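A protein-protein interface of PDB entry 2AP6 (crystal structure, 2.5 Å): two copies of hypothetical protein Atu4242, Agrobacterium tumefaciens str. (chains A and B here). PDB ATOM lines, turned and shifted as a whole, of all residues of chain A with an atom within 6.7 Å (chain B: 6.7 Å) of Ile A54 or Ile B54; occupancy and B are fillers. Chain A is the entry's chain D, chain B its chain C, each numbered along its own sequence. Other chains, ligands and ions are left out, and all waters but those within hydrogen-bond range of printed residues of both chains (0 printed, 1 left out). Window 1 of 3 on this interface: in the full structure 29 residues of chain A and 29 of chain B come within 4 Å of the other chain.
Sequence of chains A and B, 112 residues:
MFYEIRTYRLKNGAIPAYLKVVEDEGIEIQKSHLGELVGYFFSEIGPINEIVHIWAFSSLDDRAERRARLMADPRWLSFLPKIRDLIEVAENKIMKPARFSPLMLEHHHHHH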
ATOM      1  N   TYR A   3     -16.068 -24.365 -10.692  1.00  0.00           N
ATOM      2  CA  TYR A   3     -15.513 -24.103 -12.002  1.00  0.00           C
ATOM      3  C   TYR A   3     -14.113 -23.546 -11.870  1.00  0.00           C
ATOM      4  O   TYR A   3     -13.891 -22.537 -11.201  1.00  0.00           O
ATOM      5  CB  TYR A   3     -16.397 -23.124 -12.787  1.00  0.00           C
ATOM      6  CG  TYR A   3     -17.725 -23.713 -13.183  1.00  0.00           C
ATOM      7  CD1 TYR A   3     -18.781 -23.779 -12.275  1.00  0.00           C
ATOM      8  CD2 TYR A   3     -17.902 -24.283 -14.437  1.00  0.00           C
ATOM      9  CE1 TYR A   3     -19.965 -24.399 -12.596  1.00  0.00           C
ATOM     10  CE2 TYR A   3     -19.091 -24.910 -14.770  1.00  0.00           C
ATOM     11  CZ  TYR A   3     -20.111 -24.966 -13.837  1.00  0.00           C
ATOM     12  OH  TYR A   3     -21.273 -25.619 -14.133  1.00  0.00           O
ATOM     13  N   GLU A   4     -13.161 -24.229 -12.492  1.00  0.00           N
ATOM     14  CA  GLU A   4     -11.785 -23.791 -12.461  1.00  0.00           C
ATOM     15  C   GLU A   4     -11.466 -23.137 -13.792  1.00  0.00           C
ATOM     16  O   GLU A   4     -11.666 -23.732 -14.836  1.00  0.00           O
ATOM     17  CB  GLU A   4     -10.846 -24.974 -12.235  1.00  0.00           C
ATOM     18  CG  GLU A   4      -9.408 -24.674 -12.630  1.00  0.00           C
ATOM     19  CD  GLU A   4      -8.423 -25.760 -12.211  1.00  0.00           C
ATOM     20  OE1 GLU A   4      -8.816 -26.945 -12.120  1.00  0.00           O
ATOM     21  OE2 GLU A   4      -7.240 -25.429 -11.987  1.00  0.00           O
ATOM     22  N   ILE A   5     -10.986 -21.902 -13.743  1.00  0.00           N
ATOM     23  CA  ILE A   5     -10.625 -21.170 -14.951  1.00  0.00           C
ATOM     24  C   ILE A   5      -9.109 -20.970 -14.979  1.00  0.00           C
ATOM     25  O   ILE A   5      -8.534 -20.315 -14.100  1.00  0.00           O
ATOM     26  CB  ILE A   5     -11.338 -19.784 -15.005  1.00  0.00           C
ATOM     27  CG1 ILE A   5     -12.851 -19.979 -14.925  1.00  0.00           C
ATOM     28  CG2 ILE A   5     -10.985 -19.053 -16.293  1.00  0.00           C
ATOM     29  CD1 ILE A   5     -13.645 -18.709 -15.004  1.00  0.00           C
ATOM     30  N   ARG A   6      -8.461 -21.563 -15.979  1.00  0.00           N
ATOM     31  CA  ARG A   6      -7.011 -21.435 -16.120  1.00  0.00           C
ATOM     32  C   ARG A   6      -6.703 -20.543 -17.304  1.00  0.00           C
ATOM     33  O   ARG A   6      -7.230 -20.759 -18.393  1.00  0.00           O
ATOM     34  CB  ARG A   6      -6.372 -22.805 -16.319  1.00  0.00           C
ATOM     35  CG  ARG A   6      -6.677 -23.755 -15.183  1.00  0.00           C
ATOM     36  CD  ARG A   6      -6.108 -25.140 -15.454  1.00  0.00           C
ATOM     37  NE  ARG A   6      -4.649 -25.175 -15.406  1.00  0.00           N
ATOM     38  CZ  ARG A   6      -3.940 -25.270 -14.285  1.00  0.00           C
ATOM     39  NH1 ARG A   6      -4.563 -25.338 -13.110  1.00  0.00           N
ATOM     40  NH2 ARG A   6      -2.611 -25.318 -14.343  1.00  0.00           N
ATOM     41  N   GLU A  36     -15.108 -33.081 -16.692  1.00  0.00           N
ATOM     42  CA  GLU A  36     -15.857 -32.226 -17.607  1.00  0.00           C
ATOM     43  C   GLU A  36     -15.171 -30.940 -18.073  1.00  0.00           C
ATOM     44  O   GLU A  36     -14.973 -30.001 -17.296  1.00  0.00           O
ATOM     45  CB  GLU A  36     -17.207 -31.847 -16.974  1.00  0.00           C
ATOM     46  CG  GLU A  36     -18.032 -33.032 -16.474  1.00  0.00           C
ATOM     47  CD  GLU A  36     -19.187 -32.607 -15.567  1.00  0.00           C
ATOM     48  OE1 GLU A  36     -19.832 -33.498 -14.951  1.00  0.00           O
ATOM     49  OE2 GLU A  36     -19.448 -31.384 -15.476  1.00  0.00           O
ATOM     50  N   LEU A  37     -14.813 -30.902 -19.350  1.00  0.00           N
ATOM     51  CA  LEU A  37     -14.224 -29.704 -19.929  1.00  0.00           C
ATOM     52  C   LEU A  37     -15.417 -28.820 -20.301  1.00  0.00           C
ATOM     53  O   LEU A  37     -16.334 -29.263 -21.003  1.00  0.00           O
ATOM     54  CB  LEU A  37     -13.436 -30.060 -21.182  1.00  0.00           C
ATOM     55  CG  LEU A  37     -12.975 -28.883 -22.038  1.00  0.00           C
ATOM     56  CD1 LEU A  37     -12.086 -27.954 -21.218  1.00  0.00           C
ATOM     57  CD2 LEU A  37     -12.247 -29.425 -23.250  1.00  0.00           C
ATOM     58  N   VAL A  38     -15.418 -27.578 -19.830  1.00  0.00           N
ATOM     59  CA  VAL A  38     -16.518 -26.675 -20.119  1.00  0.00           C
ATOM     60  C   VAL A  38     -16.268 -25.864 -21.385  1.00  0.00           C
ATOM     61  O   VAL A  38     -17.171 -25.646 -22.186  1.00  0.00           O
ATOM     62  CB  VAL A  38     -16.769 -25.725 -18.932  1.00  0.00           C
ATOM     63  CG1 VAL A  38     -17.929 -24.799 -19.240  1.00  0.00           C
ATOM     64  CG2 VAL A  38     -17.068 -26.535 -17.684  1.00  0.00           C
ATOM     65  N   GLY A  39     -15.028 -25.431 -21.562  1.00  0.00           N
ATOM     66  CA  GLY A  39     -14.678 -24.641 -22.721  1.00  0.00           C
ATOM     67  C   GLY A  39     -13.186 -24.463 -22.807  1.00  0.00           C
ATOM     68  O   GLY A  39     -12.504 -24.450 -21.783  1.00  0.00           O
ATOM     69  N   TYR A  40     -12.685 -24.332 -24.034  1.00  0.00           N
ATOM     70  CA  TYR A  40     -11.260 -24.158 -24.293  1.00  0.00           C
ATOM     71  C   TYR A  40     -11.142 -23.111 -25.397  1.00  0.00           C
ATOM     72  O   TYR A  40     -11.507 -23.376 -26.531  1.00  0.00           O
ATOM     73  CB  TYR A  40     -10.661 -25.491 -24.744  1.00  0.00           C
ATOM     74  CG  TYR A  40      -9.231 -25.707 -24.303  1.00  0.00           C
ATOM     75  CD1 TYR A  40      -8.200 -24.892 -24.778  1.00  0.00           C
ATOM     76  CD2 TYR A  40      -8.904 -26.745 -23.418  1.00  0.00           C
ATOM     77  CE1 TYR A  40      -6.879 -25.109 -24.387  1.00  0.00           C
ATOM     78  CE2 TYR A  40      -7.589 -26.966 -23.023  1.00  0.00           C
ATOM     79  CZ  TYR A  40      -6.584 -26.145 -23.512  1.00  0.00           C
ATOM     80  OH  TYR A  40      -5.283 -26.363 -23.119  1.00  0.00           O
ATOM     81  N   PHE A  41     -10.632 -21.927 -25.048  1.00  0.00           N
ATOM     82  CA  PHE A  41     -10.522 -20.812 -25.984  1.00  0.00           C
ATOM     83  C   PHE A  41      -9.135 -20.202 -26.126  1.00  0.00           C
ATOM     84  O   PHE A  41      -8.292 -20.317 -25.243  1.00  0.00           O
ATOM     85  CB  PHE A  41     -11.471 -19.685 -25.559  1.00  0.00           C
ATOM     86  CG  PHE A  41     -12.775 -20.163 -24.985  1.00  0.00           C
ATOM     87  CD1 PHE A  41     -13.747 -20.730 -25.803  1.00  0.00           C
ATOM     88  CD2 PHE A  41     -13.014 -20.070 -23.615  1.00  0.00           C
ATOM     89  CE1 PHE A  41     -14.945 -21.201 -25.268  1.00  0.00           C
ATOM     90  CE2 PHE A  41     -14.205 -20.535 -23.059  1.00  0.00           C
ATOM     91  CZ  PHE A  41     -15.177 -21.104 -23.892  1.00  0.00           C
ATOM     92  N   VAL A  52      -7.480 -19.836 -22.538  1.00  0.00           N
ATOM     93  CA  VAL A  52      -8.401 -19.911 -21.405  1.00  0.00           C
ATOM     94  C   VAL A  52      -9.235 -21.191 -21.511  1.00  0.00           C
ATOM     95  O   VAL A  52      -9.930 -21.395 -22.509  1.00  0.00           O
ATOM     96  CB  VAL A  52      -9.381 -18.713 -21.356  1.00  0.00           C
ATOM     97  CG1 VAL A  52     -10.445 -18.973 -20.341  1.00  0.00           C
ATOM     98  CG2 VAL A  52      -8.646 -17.426 -20.984  1.00  0.00           C
ATOM     99  N   HIS A  53      -9.129 -22.065 -20.507  1.00  0.00           N
ATOM    100  CA  HIS A  53      -9.933 -23.279 -20.478  1.00  0.00           C
ATOM    101  C   HIS A  53     -10.619 -23.423 -19.124  1.00  0.00           C
ATOM    102  O   HIS A  53     -10.079 -23.038 -18.080  1.00  0.00           O
ATOM    103  CB  HIS A  53      -9.131 -24.546 -20.843  1.00  0.00           C
ATOM    104  CG  HIS A  53      -7.822 -24.704 -20.133  1.00  0.00           C
ATOM    105  ND1 HIS A  53      -7.501 -25.842 -19.427  1.00  0.00           N
ATOM    106  CD2 HIS A  53      -6.717 -23.920 -20.103  1.00  0.00           C
ATOM    107  CE1 HIS A  53      -6.257 -25.756 -18.994  1.00  0.00           C
ATOM    108  NE2 HIS A  53      -5.757 -24.599 -19.391  1.00  0.00           N
ATOM    109  N   ILE A  54     -11.834 -23.959 -19.161  1.00  0.00           N
ATOM    110  CA  ILE A  54     -12.650 -24.107 -17.960  1.00  0.00           C
ATOM    111  C   ILE A  54     -13.048 -25.545 -17.677  1.00  0.00           C
ATOM    112  O   ILE A  54     -13.522 -26.246 -18.572  1.00  0.00           O
ATOM    113  CB  ILE A  54     -13.923 -23.244 -18.094  1.00  0.00           C
ATOM    114  CG1 ILE A  54     -13.512 -21.824 -18.521  1.00  0.00           C
ATOM    115  CG2 ILE A  54     -14.686 -23.231 -16.787  1.00  0.00           C
ATOM    116  CD1 ILE A  54     -14.645 -20.944 -18.953  1.00  0.00           C
ATOM    117  N   TRP A  55     -12.838 -25.974 -16.431  1.00  0.00           N
ATOM    118  CA  TRP A  55     -13.168 -27.326 -15.992  1.00  0.00           C
ATOM    119  C   TRP A  55     -14.114 -27.292 -14.786  1.00  0.00           C
ATOM    120  O   TRP A  55     -13.942 -26.468 -13.884  1.00  0.00           O
ATOM    121  CB  TRP A  55     -11.895 -28.096 -15.623  1.00  0.00           C
ATOM    122  CG  TRP A  55     -10.906 -28.218 -16.748  1.00  0.00           C
ATOM    123  CD1 TRP A  55      -9.986 -27.284 -17.139  1.00  0.00           C
ATOM    124  CD2 TRP A  55     -10.767 -29.320 -17.655  1.00  0.00           C
ATOM    125  NE1 TRP A  55      -9.289 -27.734 -18.233  1.00  0.00           N
ATOM    126  CE2 TRP A  55      -9.744 -28.979 -18.573  1.00  0.00           C
ATOM    127  CE3 TRP A  55     -11.405 -30.562 -17.782  1.00  0.00           C
ATOM    128  CZ2 TRP A  55      -9.345 -29.833 -19.602  1.00  0.00           C
ATOM    129  CZ3 TRP A  55     -11.005 -31.417 -18.809  1.00  0.00           C
ATOM    130  CH2 TRP A  55      -9.983 -31.044 -19.704  1.00  0.00           C
ATOM    131  N   ALA A  56     -15.107 -28.184 -14.777  1.00  0.00           N
ATOM    132  CA  ALA A  56     -16.089 -28.254 -13.685  1.00  0.00           C
ATOM    133  C   ALA A  56     -15.831 -29.442 -12.744  1.00  0.00           C
ATOM    134  O   ALA A  56     -15.625 -30.576 -13.199  1.00  0.00           O
ATOM    135  CB  ALA A  56     -17.495 -28.348 -14.257  1.00  0.00           C
ATOM    136  N   LEU A 103     -24.460 -23.343 -16.709  1.00  0.00           N
ATOM    137  CA  LEU A 103     -23.423 -24.106 -16.040  1.00  0.00           C
ATOM    138  C   LEU A 103     -23.697 -24.060 -14.545  1.00  0.00           C
ATOM    139  O   LEU A 103     -23.622 -22.997 -13.918  1.00  0.00           O
ATOM    140  CB  LEU A 103     -22.056 -23.498 -16.343  1.00  0.00           C
ATOM    141  CG  LEU A 103     -21.670 -23.528 -17.817  1.00  0.00           C
ATOM    142  CD1 LEU A 103     -20.284 -22.964 -17.984  1.00  0.00           C
ATOM    143  CD2 LEU A 103     -21.724 -24.968 -18.330  1.00  0.00           C
ATOM    144  N   TYR B   3     -16.701 -16.109 -28.651  1.00  0.00           N
ATOM    145  CA  TYR B   3     -17.026 -16.130 -27.237  1.00  0.00           C
ATOM    146  C   TYR B   3     -16.583 -14.838 -26.593  1.00  0.00           C
ATOM    147  O   TYR B   3     -15.424 -14.467 -26.689  1.00  0.00           O
ATOM    148  CB  TYR B   3     -16.368 -17.327 -26.526  1.00  0.00           C
ATOM    149  CG  TYR B   3     -16.983 -18.654 -26.920  1.00  0.00           C
ATOM    150  CD1 TYR B   3     -16.635 -19.266 -28.122  1.00  0.00           C
ATOM    151  CD2 TYR B   3     -17.991 -19.237 -26.148  1.00  0.00           C
ATOM    152  CE1 TYR B   3     -17.284 -20.414 -28.558  1.00  0.00           C
ATOM    153  CE2 TYR B   3     -18.644 -20.388 -26.573  1.00  0.00           C
ATOM    154  CZ  TYR B   3     -18.282 -20.962 -27.788  1.00  0.00           C
ATOM    155  OH  TYR B   3     -18.944 -22.057 -28.266  1.00  0.00           O
ATOM    156  N   GLU B   4     -17.518 -14.144 -25.955  1.00  0.00           N
ATOM    157  CA  GLU B   4     -17.195 -12.901 -25.276  1.00  0.00           C
ATOM    158  C   GLU B   4     -17.126 -13.175 -23.793  1.00  0.00           C
ATOM    159  O   GLU B   4     -18.058 -13.719 -23.221  1.00  0.00           O
ATOM    160  CB  GLU B   4     -18.250 -11.819 -25.548  1.00  0.00           C
ATOM    161  CG  GLU B   4     -18.172 -10.655 -24.564  1.00  0.00           C
ATOM    162  CD  GLU B   4     -19.113  -9.509 -24.889  1.00  0.00           C
ATOM    163  OE1 GLU B   4     -20.184  -9.751 -25.487  1.00  0.00           O
ATOM    164  OE2 GLU B   4     -18.782  -8.359 -24.524  1.00  0.00           O
ATOM    165  N   ILE B   5     -16.011 -12.809 -23.176  1.00  0.00           N
ATOM    166  CA  ILE B   5     -15.843 -13.016 -21.748  1.00  0.00           C
ATOM    167  C   ILE B   5     -15.753 -11.663 -21.064  1.00  0.00           C
ATOM    168  O   ILE B   5     -14.858 -10.871 -21.337  1.00  0.00           O
ATOM    169  CB  ILE B   5     -14.574 -13.843 -21.439  1.00  0.00           C
ATOM    170  CG1 ILE B   5     -14.644 -15.191 -22.162  1.00  0.00           C
ATOM    171  CG2 ILE B   5     -14.436 -14.048 -19.950  1.00  0.00           C
ATOM    172  CD1 ILE B   5     -13.438 -16.097 -21.928  1.00  0.00           C
ATOM    173  N   ARG B   6     -16.713 -11.395 -20.192  1.00  0.00           N
ATOM    174  CA  ARG B   6     -16.749 -10.137 -19.464  1.00  0.00           C
ATOM    175  C   ARG B   6     -16.410 -10.410 -18.007  1.00  0.00           C
ATOM    176  O   ARG B   6     -16.966 -11.311 -17.383  1.00  0.00           O
ATOM    177  CB  ARG B   6     -18.134  -9.483 -19.588  1.00  0.00           C
ATOM    178  CG  ARG B   6     -18.582  -9.259 -21.026  1.00  0.00           C
ATOM    179  CD  ARG B   6     -20.009  -8.738 -21.075  1.00  0.00           C
ATOM    180  NE  ARG B   6     -20.106  -7.372 -20.573  1.00  0.00           N
ATOM    181  CZ  ARG B   6     -19.759  -6.297 -21.275  1.00  0.00           C
ATOM    182  NH1 ARG B   6     -19.299  -6.440 -22.504  1.00  0.00           N
ATOM    183  NH2 ARG B   6     -19.872  -5.083 -20.751  1.00  0.00           N
ATOM    184  N   GLU B  36     -27.130 -16.739 -26.590  1.00  0.00           N
ATOM    185  CA  GLU B  36     -26.669 -17.860 -25.780  1.00  0.00           C
ATOM    186  C   GLU B  36     -25.714 -17.519 -24.648  1.00  0.00           C
ATOM    187  O   GLU B  36     -24.579 -17.101 -24.880  1.00  0.00           O
ATOM    188  CB  GLU B  36     -26.001 -18.917 -26.667  1.00  0.00           C
ATOM    189  CG  GLU B  36     -26.854 -19.373 -27.849  1.00  0.00           C
ATOM    190  CD  GLU B  36     -26.035 -20.096 -28.917  1.00  0.00           C
ATOM    191  OE1 GLU B  36     -26.608 -20.435 -29.994  1.00  0.00           O
ATOM    192  OE2 GLU B  36     -24.817 -20.332 -28.677  1.00  0.00           O
ATOM    193  N   LEU B  37     -26.186 -17.707 -23.420  1.00  0.00           N
ATOM    194  CA  LEU B  37     -25.365 -17.488 -22.238  1.00  0.00           C
ATOM    195  C   LEU B  37     -24.619 -18.803 -22.052  1.00  0.00           C
ATOM    196  O   LEU B  37     -25.232 -19.863 -21.984  1.00  0.00           O
ATOM    197  CB  LEU B  37     -26.238 -17.212 -21.015  1.00  0.00           C
ATOM    198  CG  LEU B  37     -25.507 -17.179 -19.666  1.00  0.00           C
ATOM    199  CD1 LEU B  37     -24.470 -16.078 -19.662  1.00  0.00           C
ATOM    200  CD2 LEU B  37     -26.504 -16.971 -18.545  1.00  0.00           C
ATOM    201  N   VAL B  38     -23.293 -18.737 -21.985  1.00  0.00           N
ATOM    202  CA  VAL B  38     -22.480 -19.939 -21.826  1.00  0.00           C
ATOM    203  C   VAL B  38     -22.241 -20.294 -20.346  1.00  0.00           C
ATOM    204  O   VAL B  38     -22.247 -21.463 -19.954  1.00  0.00           O
ATOM    205  CB  VAL B  38     -21.117 -19.774 -22.556  1.00  0.00           C
ATOM    206  CG1 VAL B  38     -20.306 -21.031 -22.417  1.00  0.00           C
ATOM    207  CG2 VAL B  38     -21.336 -19.473 -24.013  1.00  0.00           C
ATOM    208  N   GLY B  39     -22.041 -19.264 -19.531  1.00  0.00           N
ATOM    209  CA  GLY B  39     -21.798 -19.463 -18.116  1.00  0.00           C
ATOM    210  C   GLY B  39     -21.741 -18.134 -17.401  1.00  0.00           C
ATOM    211  O   GLY B  39     -21.355 -17.121 -17.986  1.00  0.00           O
ATOM    212  N   TYR B  40     -22.138 -18.143 -16.135  1.00  0.00           N
ATOM    213  CA  TYR B  40     -22.162 -16.947 -15.303  1.00  0.00           C
ATOM    214  C   TYR B  40     -21.619 -17.356 -13.933  1.00  0.00           C
ATOM    215  O   TYR B  40     -22.265 -18.098 -13.208  1.00  0.00           O
ATOM    216  CB  TYR B  40     -23.610 -16.439 -15.184  1.00  0.00           C
ATOM    217  CG  TYR B  40     -23.740 -14.929 -15.076  1.00  0.00           C
ATOM    218  CD1 TYR B  40     -23.275 -14.242 -13.948  1.00  0.00           C
ATOM    219  CD2 TYR B  40     -24.336 -14.185 -16.099  1.00  0.00           C
ATOM    220  CE1 TYR B  40     -23.407 -12.850 -13.848  1.00  0.00           C
ATOM    221  CE2 TYR B  40     -24.471 -12.797 -16.004  1.00  0.00           C
ATOM    222  CZ  TYR B  40     -24.006 -12.142 -14.881  1.00  0.00           C
ATOM    223  OH  TYR B  40     -24.130 -10.782 -14.795  1.00  0.00           O
ATOM    224  N   PHE B  41     -20.430 -16.867 -13.586  1.00  0.00           N
ATOM    225  CA  PHE B  41     -19.792 -17.236 -12.329  1.00  0.00           C
ATOM    226  C   PHE B  41     -19.398 -16.069 -11.444  1.00  0.00           C
ATOM    227  O   PHE B  41     -19.252 -14.942 -11.902  1.00  0.00           O
ATOM    228  CB  PHE B  41     -18.530 -18.052 -12.611  1.00  0.00           C
ATOM    229  CG  PHE B  41     -18.654 -18.972 -13.781  1.00  0.00           C
ATOM    230  CD1 PHE B  41     -19.350 -20.175 -13.670  1.00  0.00           C
ATOM    231  CD2 PHE B  41     -18.091 -18.629 -15.018  1.00  0.00           C
ATOM    232  CE1 PHE B  41     -19.485 -21.021 -14.767  1.00  0.00           C
ATOM    233  CE2 PHE B  41     -18.221 -19.470 -16.123  1.00  0.00           C
ATOM    234  CZ  PHE B  41     -18.917 -20.667 -15.997  1.00  0.00           C
ATOM    235  N   VAL B  52     -17.784 -13.183 -13.683  1.00  0.00           N
ATOM    236  CA  VAL B  52     -17.337 -13.583 -15.001  1.00  0.00           C
ATOM    237  C   VAL B  52     -18.487 -14.279 -15.718  1.00  0.00           C
ATOM    238  O   VAL B  52     -19.000 -15.286 -15.236  1.00  0.00           O
ATOM    239  CB  VAL B  52     -16.153 -14.568 -14.920  1.00  0.00           C
ATOM    240  CG1 VAL B  52     -15.921 -15.241 -16.272  1.00  0.00           C
ATOM    241  CG2 VAL B  52     -14.907 -13.837 -14.467  1.00  0.00           C
ATOM    242  N   HIS B  53     -18.911 -13.726 -16.853  1.00  0.00           N
ATOM    243  CA  HIS B  53     -19.961 -14.345 -17.645  1.00  0.00           C
ATOM    244  C   HIS B  53     -19.522 -14.424 -19.099  1.00  0.00           C
ATOM    245  O   HIS B  53     -18.819 -13.552 -19.603  1.00  0.00           O
ATOM    246  CB  HIS B  53     -21.323 -13.629 -17.489  1.00  0.00           C
ATOM    247  CG  HIS B  53     -21.282 -12.143 -17.654  1.00  0.00           C
ATOM    248  ND1 HIS B  53     -22.113 -11.473 -18.529  1.00  0.00           N
ATOM    249  CD2 HIS B  53     -20.574 -11.187 -17.003  1.00  0.00           C
ATOM    250  CE1 HIS B  53     -21.920 -10.171 -18.413  1.00  0.00           C
ATOM    251  NE2 HIS B  53     -20.992  -9.971 -17.494  1.00  0.00           N
ATOM    252  N   ILE B  54     -19.924 -15.505 -19.756  1.00  0.00           N
ATOM    253  CA  ILE B  54     -19.549 -15.758 -21.143  1.00  0.00           C
ATOM    254  C   ILE B  54     -20.743 -15.902 -22.089  1.00  0.00           C
ATOM    255  O   ILE B  54     -21.693 -16.640 -21.814  1.00  0.00           O
ATOM    256  CB  ILE B  54     -18.695 -17.039 -21.226  1.00  0.00           C
ATOM    257  CG1 ILE B  54     -17.625 -17.003 -20.133  1.00  0.00           C
ATOM    258  CG2 ILE B  54     -18.062 -17.151 -22.599  1.00  0.00           C
ATOM    259  CD1 ILE B  54     -16.889 -18.301 -19.931  1.00  0.00           C
ATOM    260  N   TRP B  55     -20.678 -15.186 -23.210  1.00  0.00           N
ATOM    261  CA  TRP B  55     -21.733 -15.217 -24.219  1.00  0.00           C
ATOM    262  C   TRP B  55     -21.166 -15.613 -25.583  1.00  0.00           C
ATOM    263  O   TRP B  55     -20.091 -15.152 -25.970  1.00  0.00           O
ATOM    264  CB  TRP B  55     -22.411 -13.845 -24.333  1.00  0.00           C
ATOM    265  CG  TRP B  55     -23.020 -13.356 -23.053  1.00  0.00           C
ATOM    266  CD1 TRP B  55     -22.366 -12.782 -21.991  1.00  0.00           C
ATOM    267  CD2 TRP B  55     -24.392 -13.451 -22.672  1.00  0.00           C
ATOM    268  NE1 TRP B  55     -23.251 -12.524 -20.975  1.00  0.00           N
ATOM    269  CE2 TRP B  55     -24.501 -12.924 -21.365  1.00  0.00           C
ATOM    270  CE3 TRP B  55     -25.544 -13.931 -23.309  1.00  0.00           C
ATOM    271  CZ2 TRP B  55     -25.717 -12.867 -20.679  1.00  0.00           C
ATOM    272  CZ3 TRP B  55     -26.752 -13.873 -22.630  1.00  0.00           C
ATOM    273  CH2 TRP B  55     -26.829 -13.342 -21.322  1.00  0.00           C
ATOM    274  N   ALA B  56     -21.893 -16.459 -26.309  1.00  0.00           N
ATOM    275  CA  ALA B  56     -21.466 -16.904 -27.638  1.00  0.00           C
ATOM    276  C   ALA B  56     -22.206 -16.160 -28.765  1.00  0.00           C
ATOM    277  O   ALA B  56     -23.430 -15.995 -28.716  1.00  0.00           O
ATOM    278  CB  ALA B  56     -21.691 -18.401 -27.785  1.00  0.00           C
ATOM    279  N   LEU B 103     -17.536 -26.203 -26.489  1.00  0.00           N
ATOM    280  CA  LEU B 103     -18.055 -24.926 -26.959  1.00  0.00           C
ATOM    281  C   LEU B 103     -17.416 -24.618 -28.306  1.00  0.00           C
ATOM    282  O   LEU B 103     -16.202 -24.409 -28.409  1.00  0.00           O
ATOM    283  CB  LEU B 103     -17.742 -23.814 -25.948  1.00  0.00           C
ATOM    284  CG  LEU B 103     -18.363 -24.053 -24.557  1.00  0.00           C
ATOM    285  CD1 LEU B 103     -18.008 -22.906 -23.641  1.00  0.00           C
ATOM    286  CD2 LEU B 103     -19.888 -24.211 -24.676  1.00  0.00           C
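Phe B41 touches Tyr A3 (CE1 to CG, 3.6 Å). O of Val A38 touches CG of Leu B103, at 3.1 Å. CD1 of Leu B103 touches CA of Gly A39, at 3.9 Å. Phe A41 touches Tyr B3. CZ of Phe A41 touches CD1 of Leu B103, 3.4 Å away. CD1 of Ile B54 touches CD1 of Ile A54 (3.6 Å). Leu A103 touches Val B38 (CG to O, 3.0 Å). CD1 of Leu A103 touches CA of Gly B39, at 3.8 Å. Leu A103 touches Phe B41 (CD1 to CZ, 3.3 Å).
The backbone carbonyl oxygen (O) of Gly B39 lies within hydrogen-bond range of the backbone NH (N) of Ile B54. The backbone NH of Phe B41 sits at hydrogen-bond distance from the backbone carbonyl oxygen of Val B52, 2.7 Å away. The backbone carbonyl oxygen of Ile A54 lies within hydrogen-bond range of the backbone NH of Val A38 (2.6 Å). The backbone carbonyl oxygen (O) of Ile B54 sits at hydrogen-bond distance from the backbone NH (N) of Val B38, 2.6 Å away. N of Phe A41 is in hydrogen-bond range of O of Val A52 (2.7 Å). The backbone carbonyl oxygen (O) of Gly A39 lies within hydrogen-bond range of the backbone NH (N) of Ile A54, 2.8 Å away.
Tyr A3 touches Phe B41, and with the chains exchanged Phe A41 touches Tyr B3. Val A38 touches Leu B103, and with the chains exchanged Leu A103 touches Val B38. Phe A41 touches Leu B103, and with the chains exchanged Leu A103 touches Phe B41. Ile B54 touches its own counterpart, Ile A54. Of the 9 pairs that touch across the chains among the printed residues, 9 have their exchanged pair printed and touching as well.
Of the 16 printed residues of chain A, 6 touch a printed residue of chain B. Hydrophobic or aromatic side chains of chain A within 4 Å of the printed part of chain B: Tyr A3, Phe A41, Ile A54 and Leu A103. Among the printed residues, no Asp or Glu carboxylate lies within 4 Å of a Lys or Arg side-chain nitrogen of the other chain.
Ile A54 touches just one residue of chain B: Ile B54 (3.6 Å). Ile B54 touches one residue of chain A. Of the printed residues of chain B, Tyr A3 touches Phe B41. Of the printed residues of chain B, Val A38 touches Leu B103. Of the printed residues of chain A, Phe B41 touches Tyr A3 and Leu A103. His B53 touches none of the printed residues of chain A. Ile B5 touches none of the printed residues of chain A. The nearest residue of chain B that does not touch Ile A54 is Phe B41 (4.8 Å). The nearest printed residue of chain B that does not touch Phe A41 is Ile B5 (4.3 Å).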
